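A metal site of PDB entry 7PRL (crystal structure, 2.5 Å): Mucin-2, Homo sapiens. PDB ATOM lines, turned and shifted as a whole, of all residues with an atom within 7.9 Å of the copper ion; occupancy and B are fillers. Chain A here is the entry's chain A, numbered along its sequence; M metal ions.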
ATOM      1  N   HIS A  32     -20.491  -7.961   8.696  1.00  0.00           N
ATOM      2  CA  HIS A  32     -20.619  -6.909   7.690  1.00  0.00           C
ATOM      3  C   HIS A  32     -21.234  -7.499   6.427  1.00  0.00           C
ATOM      4  O   HIS A  32     -20.698  -8.457   5.859  1.00  0.00           O
ATOM      5  CB  HIS A  32     -19.266  -6.269   7.374  1.00  0.00           C
ATOM      6  N   GLY A  33     -22.347  -6.907   5.987  1.00  0.00           N
ATOM      7  CA  GLY A  33     -23.139  -7.471   4.915  1.00  0.00           C
ATOM      8  C   GLY A  33     -22.805  -6.901   3.545  1.00  0.00           C
ATOM      9  O   GLY A  33     -21.862  -6.143   3.354  1.00  0.00           O
ATOM     10  N   HIS A  34     -23.601  -7.308   2.575  1.00  0.00           N
ATOM     11  CA  HIS A  34     -23.449  -6.866   1.207  1.00  0.00           C
ATOM     12  C   HIS A  34     -24.810  -6.479   0.651  1.00  0.00           C
ATOM     13  O   HIS A  34     -25.855  -6.824   1.224  1.00  0.00           O
ATOM     14  CB  HIS A  34     -22.766  -7.955   0.359  1.00  0.00           C
ATOM     15  CG  HIS A  34     -21.275  -7.943   0.462  1.00  0.00           C
ATOM     16  ND1 HIS A  34     -20.497  -9.064   0.263  1.00  0.00           N
ATOM     17  CD2 HIS A  34     -20.412  -6.930   0.747  1.00  0.00           C
ATOM     18  CE1 HIS A  34     -19.224  -8.749   0.415  1.00  0.00           C
ATOM     19  NE2 HIS A  34     -19.144  -7.464   0.706  1.00  0.00           N
ATOM     20  N   ASN A  35     -24.800  -5.750  -0.458  1.00  0.00           N
ATOM     21  CA  ASN A  35     -26.027  -5.313  -1.128  1.00  0.00           C
ATOM     22  C   ASN A  35     -26.212  -6.196  -2.361  1.00  0.00           C
ATOM     23  O   ASN A  35     -25.506  -6.060  -3.357  1.00  0.00           O
ATOM     24  CB  ASN A  35     -25.940  -3.836  -1.482  1.00  0.00           C
ATOM     25  CG  ASN A  35     -26.071  -2.961  -0.267  1.00  0.00           C
ATOM     26  OD1 ASN A  35     -25.247  -2.078  -0.045  1.00  0.00           O
ATOM     27  ND2 ASN A  35     -27.103  -3.218   0.550  1.00  0.00           N
ATOM     28  N   VAL A  36     -27.141  -7.129  -2.272  1.00  0.00           N
ATOM     29  CA  VAL A  36     -27.185  -8.222  -3.220  1.00  0.00           C
ATOM     30  C   VAL A  36     -28.537  -8.225  -3.908  1.00  0.00           C
ATOM     31  O   VAL A  36     -29.572  -7.902  -3.317  1.00  0.00           O
ATOM     32  CB  VAL A  36     -26.914  -9.582  -2.530  1.00  0.00           C
ATOM     33  CG1 VAL A  36     -25.493  -9.626  -1.975  1.00  0.00           C
ATOM     34  CG2 VAL A  36     -27.919  -9.865  -1.426  1.00  0.00           C
ATOM     35  N   THR A 144     -19.158  -7.832  -7.797  1.00  0.00           N
ATOM     36  CA  THR A 144     -18.857  -9.249  -7.630  1.00  0.00           C
ATOM     37  C   THR A 144     -20.066 -10.066  -8.060  1.00  0.00           C
ATOM     38  O   THR A 144     -21.204  -9.708  -7.743  1.00  0.00           O
ATOM     39  CB  THR A 144     -18.474  -9.575  -6.152  1.00  0.00           C
ATOM     40  OG1 THR A 144     -17.292  -8.840  -5.809  1.00  0.00           O
ATOM     41  CG2 THR A 144     -18.222 -11.072  -5.908  1.00  0.00           C
ATOM     42  N   MET A 146     -21.663 -14.206  -8.563  1.00  0.00           N
ATOM     43  CA  MET A 146     -21.576 -15.611  -8.191  1.00  0.00           C
ATOM     44  C   MET A 146     -22.757 -16.400  -8.770  1.00  0.00           C
ATOM     45  O   MET A 146     -23.913 -16.083  -8.473  1.00  0.00           O
ATOM     46  CB  MET A 146     -21.588 -15.759  -6.691  1.00  0.00           C
ATOM     47  CG  MET A 146     -20.294 -15.378  -6.032  1.00  0.00           C
ATOM     48  SD  MET A 146     -20.541 -15.264  -4.270  1.00  0.00           S
ATOM     49  CE  MET A 146     -19.255 -14.091  -3.865  1.00  0.00           C
ATOM     50  N   MET A 154     -26.335 -14.362  -8.408  1.00  0.00           N
ATOM     51  CA  MET A 154     -26.307 -13.366  -7.350  1.00  0.00           C
ATOM     52  C   MET A 154     -25.255 -12.301  -7.616  1.00  0.00           C
ATOM     53  O   MET A 154     -24.118 -12.624  -7.964  1.00  0.00           O
ATOM     54  CB  MET A 154     -26.034 -14.071  -6.048  1.00  0.00           C
ATOM     55  CG  MET A 154     -25.750 -13.184  -4.921  1.00  0.00           C
ATOM     56  SD  MET A 154     -25.873 -14.240  -3.488  1.00  0.00           S
ATOM     57  CE  MET A 154     -26.888 -13.159  -2.486  1.00  0.00           C
ATOM     58  N   LEU A 155     -25.636 -11.023  -7.433  1.00  0.00           N
ATOM     59  CA  LEU A 155     -24.765  -9.900  -7.761  1.00  0.00           C
ATOM     60  C   LEU A 155     -24.686  -8.943  -6.582  1.00  0.00           C
ATOM     61  O   LEU A 155     -25.711  -8.383  -6.170  1.00  0.00           O
ATOM     62  CB  LEU A 155     -25.277  -9.181  -9.008  1.00  0.00           C
ATOM     63  CG  LEU A 155     -24.545  -7.945  -9.499  1.00  0.00           C
ATOM     64  CD1 LEU A 155     -23.246  -8.304 -10.184  1.00  0.00           C
ATOM     65  CD2 LEU A 155     -25.472  -7.220 -10.470  1.00  0.00           C
ATOM     66  N   GLU A 156     -23.457  -8.762  -6.043  1.00  0.00           N
ATOM     67  CA  GLU A 156     -23.140  -7.747  -5.035  1.00  0.00           C
ATOM     68  C   GLU A 156     -22.604  -6.493  -5.715  1.00  0.00           C
ATOM     69  O   GLU A 156     -21.681  -6.590  -6.533  1.00  0.00           O
ATOM     70  CB  GLU A 156     -22.065  -8.230  -4.041  1.00  0.00           C
ATOM     71  CG  GLU A 156     -22.154  -9.679  -3.495  1.00  0.00           C
ATOM     72  CD  GLU A 156     -20.830 -10.200  -2.831  1.00  0.00           C
ATOM     73  OE1 GLU A 156     -19.705  -9.786  -3.232  1.00  0.00           O
ATOM     74  OE2 GLU A 156     -20.888 -11.043  -1.903  1.00  0.00           O
ATOM     75  N   ARG A 273     -28.370 -18.399   2.003  1.00  0.00           N
ATOM     76  CA  ARG A 273     -27.451 -17.493   1.300  1.00  0.00           C
ATOM     77  C   ARG A 273     -27.679 -16.038   1.711  1.00  0.00           C
ATOM     78  O   ARG A 273     -26.711 -15.284   1.880  1.00  0.00           O
ATOM     79  CB  ARG A 273     -27.620 -17.642  -0.219  1.00  0.00           C
ATOM     80  CG  ARG A 273     -27.046 -18.917  -0.835  1.00  0.00           C
ATOM     81  CD  ARG A 273     -26.939 -18.848  -2.378  1.00  0.00           C
ATOM     82  NE  ARG A 273     -28.251 -18.999  -3.012  1.00  0.00           N
ATOM     83  CZ  ARG A 273     -28.871 -20.163  -3.188  1.00  0.00           C
ATOM     84  NH1 ARG A 273     -28.312 -21.282  -2.774  1.00  0.00           N
ATOM     85  NH2 ARG A 273     -30.065 -20.205  -3.739  1.00  0.00           N
ATOM     86  N   GLN A 274     -28.929 -15.623   1.856  1.00  0.00           N
ATOM     87  CA  GLN A 274     -29.184 -14.229   2.236  1.00  0.00           C
ATOM     88  C   GLN A 274     -28.655 -13.934   3.637  1.00  0.00           C
ATOM     89  O   GLN A 274     -28.154 -12.838   3.896  1.00  0.00           O
ATOM     90  CB  GLN A 274     -30.676 -13.904   2.154  1.00  0.00           C
ATOM     91  CG  GLN A 274     -31.181 -13.729   0.744  1.00  0.00           C
ATOM     92  CD  GLN A 274     -30.402 -12.681  -0.063  1.00  0.00           C
ATOM     93  OE1 GLN A 274     -30.136 -12.889  -1.257  1.00  0.00           O
ATOM     94  NE2 GLN A 274     -30.070 -11.548   0.579  1.00  0.00           N
ATOM     95  N   SER A 276     -26.001 -15.363   5.084  1.00  0.00           N
ATOM     96  CA  SER A 276     -24.554 -15.220   4.963  1.00  0.00           C
ATOM     97  C   SER A 276     -24.171 -13.883   4.361  1.00  0.00           C
ATOM     98  O   SER A 276     -23.254 -13.205   4.857  1.00  0.00           O
ATOM     99  CB  SER A 276     -23.977 -16.374   4.121  1.00  0.00           C
ATOM    100  OG  SER A 276     -24.253 -17.626   4.694  1.00  0.00           O
ATOM    101  N   HIS A 277     -24.848 -13.463   3.289  1.00  0.00           N
ATOM    102  CA  HIS A 277     -24.496 -12.184   2.674  1.00  0.00           C
ATOM    103  C   HIS A 277     -24.875 -10.975   3.535  1.00  0.00           C
ATOM    104  O   HIS A 277     -24.395  -9.872   3.249  1.00  0.00           O
ATOM    105  CB  HIS A 277     -25.143 -12.058   1.291  1.00  0.00           C
ATOM    106  CG  HIS A 277     -24.381 -12.794   0.244  1.00  0.00           C
ATOM    107  ND1 HIS A 277     -23.221 -12.303  -0.314  1.00  0.00           N
ATOM    108  CD2 HIS A 277     -24.545 -14.033  -0.283  1.00  0.00           C
ATOM    109  CE1 HIS A 277     -22.745 -13.175  -1.169  1.00  0.00           C
ATOM    110  NE2 HIS A 277     -23.524 -14.244  -1.167  1.00  0.00           N
ATOM    111  N   ALA A 278     -25.687 -11.166   4.567  1.00  0.00           N
ATOM    112  CA  ALA A 278     -26.016 -10.098   5.501  1.00  0.00           C
ATOM    113  C   ALA A 278     -25.160 -10.141   6.770  1.00  0.00           C
ATOM    114  O   ALA A 278     -25.557  -9.565   7.785  1.00  0.00           O
ATOM    115  CB  ALA A 278     -27.494 -10.152   5.863  1.00  0.00           C
ATOM    116  N   GLY A 279     -24.007 -10.842   6.734  1.00  0.00           N
ATOM    117  CA  GLY A 279     -23.082 -10.912   7.849  1.00  0.00           C
ATOM    118  C   GLY A 279     -23.320 -12.011   8.869  1.00  0.00           C
ATOM    119  O   GLY A 279     -22.531 -12.137   9.821  1.00  0.00           O
ATOM    120  N   GLU A 323     -13.852 -10.912   4.023  1.00  0.00           N
ATOM    121  CA  GLU A 323     -15.294 -10.799   3.841  1.00  0.00           C
ATOM    122  C   GLU A 323     -16.023 -11.876   4.640  1.00  0.00           C
ATOM    123  O   GLU A 323     -15.416 -12.713   5.311  1.00  0.00           O
ATOM    124  CB  GLU A 323     -15.662 -10.891   2.353  1.00  0.00           C
ATOM    125  CG  GLU A 323     -14.992  -9.878   1.458  1.00  0.00           C
ATOM    126  CD  GLU A 323     -15.895  -8.717   1.126  1.00  0.00           C
ATOM    127  OE1 GLU A 323     -16.384  -8.058   2.077  1.00  0.00           O
ATOM    128  OE2 GLU A 323     -16.119  -8.472  -0.094  1.00  0.00           O
ATOM    129  N   HIS A 324     -17.355 -11.880   4.538  1.00  0.00           N
ATOM    130  CA  HIS A 324     -18.183 -12.827   5.262  1.00  0.00           C
ATOM    131  C   HIS A 324     -18.004 -14.232   4.706  1.00  0.00           C
ATOM    132  O   HIS A 324     -17.494 -14.427   3.603  1.00  0.00           O
ATOM    133  CB  HIS A 324     -19.659 -12.421   5.211  1.00  0.00           C
ATOM    134  CG  HIS A 324     -20.244 -12.389   3.822  1.00  0.00           C
ATOM    135  ND1 HIS A 324     -20.825 -13.487   3.235  1.00  0.00           N
ATOM    136  CD2 HIS A 324     -20.340 -11.376   2.926  1.00  0.00           C
ATOM    137  CE1 HIS A 324     -21.247 -13.165   2.025  1.00  0.00           C
ATOM    138  NE2 HIS A 324     -20.973 -11.891   1.813  1.00  0.00           N
ATOM    139  N   ARG A 325     -18.407 -15.228   5.517  1.00  0.00           N
ATOM    140  CA  ARG A 325     -18.340 -16.636   5.183  1.00  0.00           C
ATOM    141  C   ARG A 325     -19.499 -17.006   4.244  1.00  0.00           C
ATOM    142  O   ARG A 325     -20.507 -16.310   4.173  1.00  0.00           O
ATOM    143  CB  ARG A 325     -18.377 -17.490   6.459  1.00  0.00           C
ATOM    144  CG  ARG A 325     -17.139 -17.352   7.361  1.00  0.00           C
ATOM    145  CD  ARG A 325     -17.274 -18.107   8.712  1.00  0.00           C
ATOM    146  NE  ARG A 325     -16.934 -19.521   8.612  1.00  0.00           N
ATOM    147  CZ  ARG A 325     -15.689 -20.017   8.625  1.00  0.00           C
ATOM    148  NH1 ARG A 325     -14.637 -19.215   8.761  1.00  0.00           N
ATOM    149  NH2 ARG A 325     -15.499 -21.320   8.514  1.00  0.00           N
ATOM    150  N   MET A 326     -19.321 -18.123   3.515  1.00  0.00           N
ATOM    151  CA  MET A 326     -20.261 -18.544   2.464  1.00  0.00           C
ATOM    152  C   MET A 326     -20.335 -20.068   2.392  1.00  0.00           C
ATOM    153  O   MET A 326     -19.414 -20.779   2.807  1.00  0.00           O
ATOM    154  CB  MET A 326     -19.847 -18.068   1.073  1.00  0.00           C
ATOM    155  CG  MET A 326     -20.228 -16.694   0.699  1.00  0.00           C
ATOM    156  SD  MET A 326     -19.801 -16.548  -1.036  1.00  0.00           S
ATOM    157  CE  MET A 326     -20.871 -17.798  -1.753  1.00  0.00           C
HETATM  158 CU    CU M   1     -21.817 -10.925   0.157  1.00  0.00          CU
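Within 4 Å of the copper ion: His 34, Glu 156, His 277 and His 324.
The nearest printed residue that does not touch the copper ion is Val 36 (4.4 Å).
The copper ion is bound by a ring nitrogen (ND1) of His 277 (2.0 Å), a ring nitrogen (NE2) of His 324 (2.1 Å), the side-chain carboxylate of Glu 156 (2.3 Å) and a ring nitrogen (ND1) of His 34 (2.3 Å).
The copper ion has four donor atoms within binding distance.
The backbone carbonyl oxygen (O) of Thr 144 lies within hydrogen-bond range of the backbone NH (N) of Glu 156, 3.0 Å away.
The side-chain carboxylate (OE1) of Glu 323 is in hydrogen-bond range of a ring nitrogen (NE2) of His 34 (3.1 Å).
A ring nitrogen (NE2) of His 277 is in hydrogen-bond range of the side-chain sulfur of Met 154 (3.3 Å).
A ring nitrogen (ND1) of His 324 is in hydrogen-bond range of the backbone carbonyl oxygen (O) of Ser 276.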
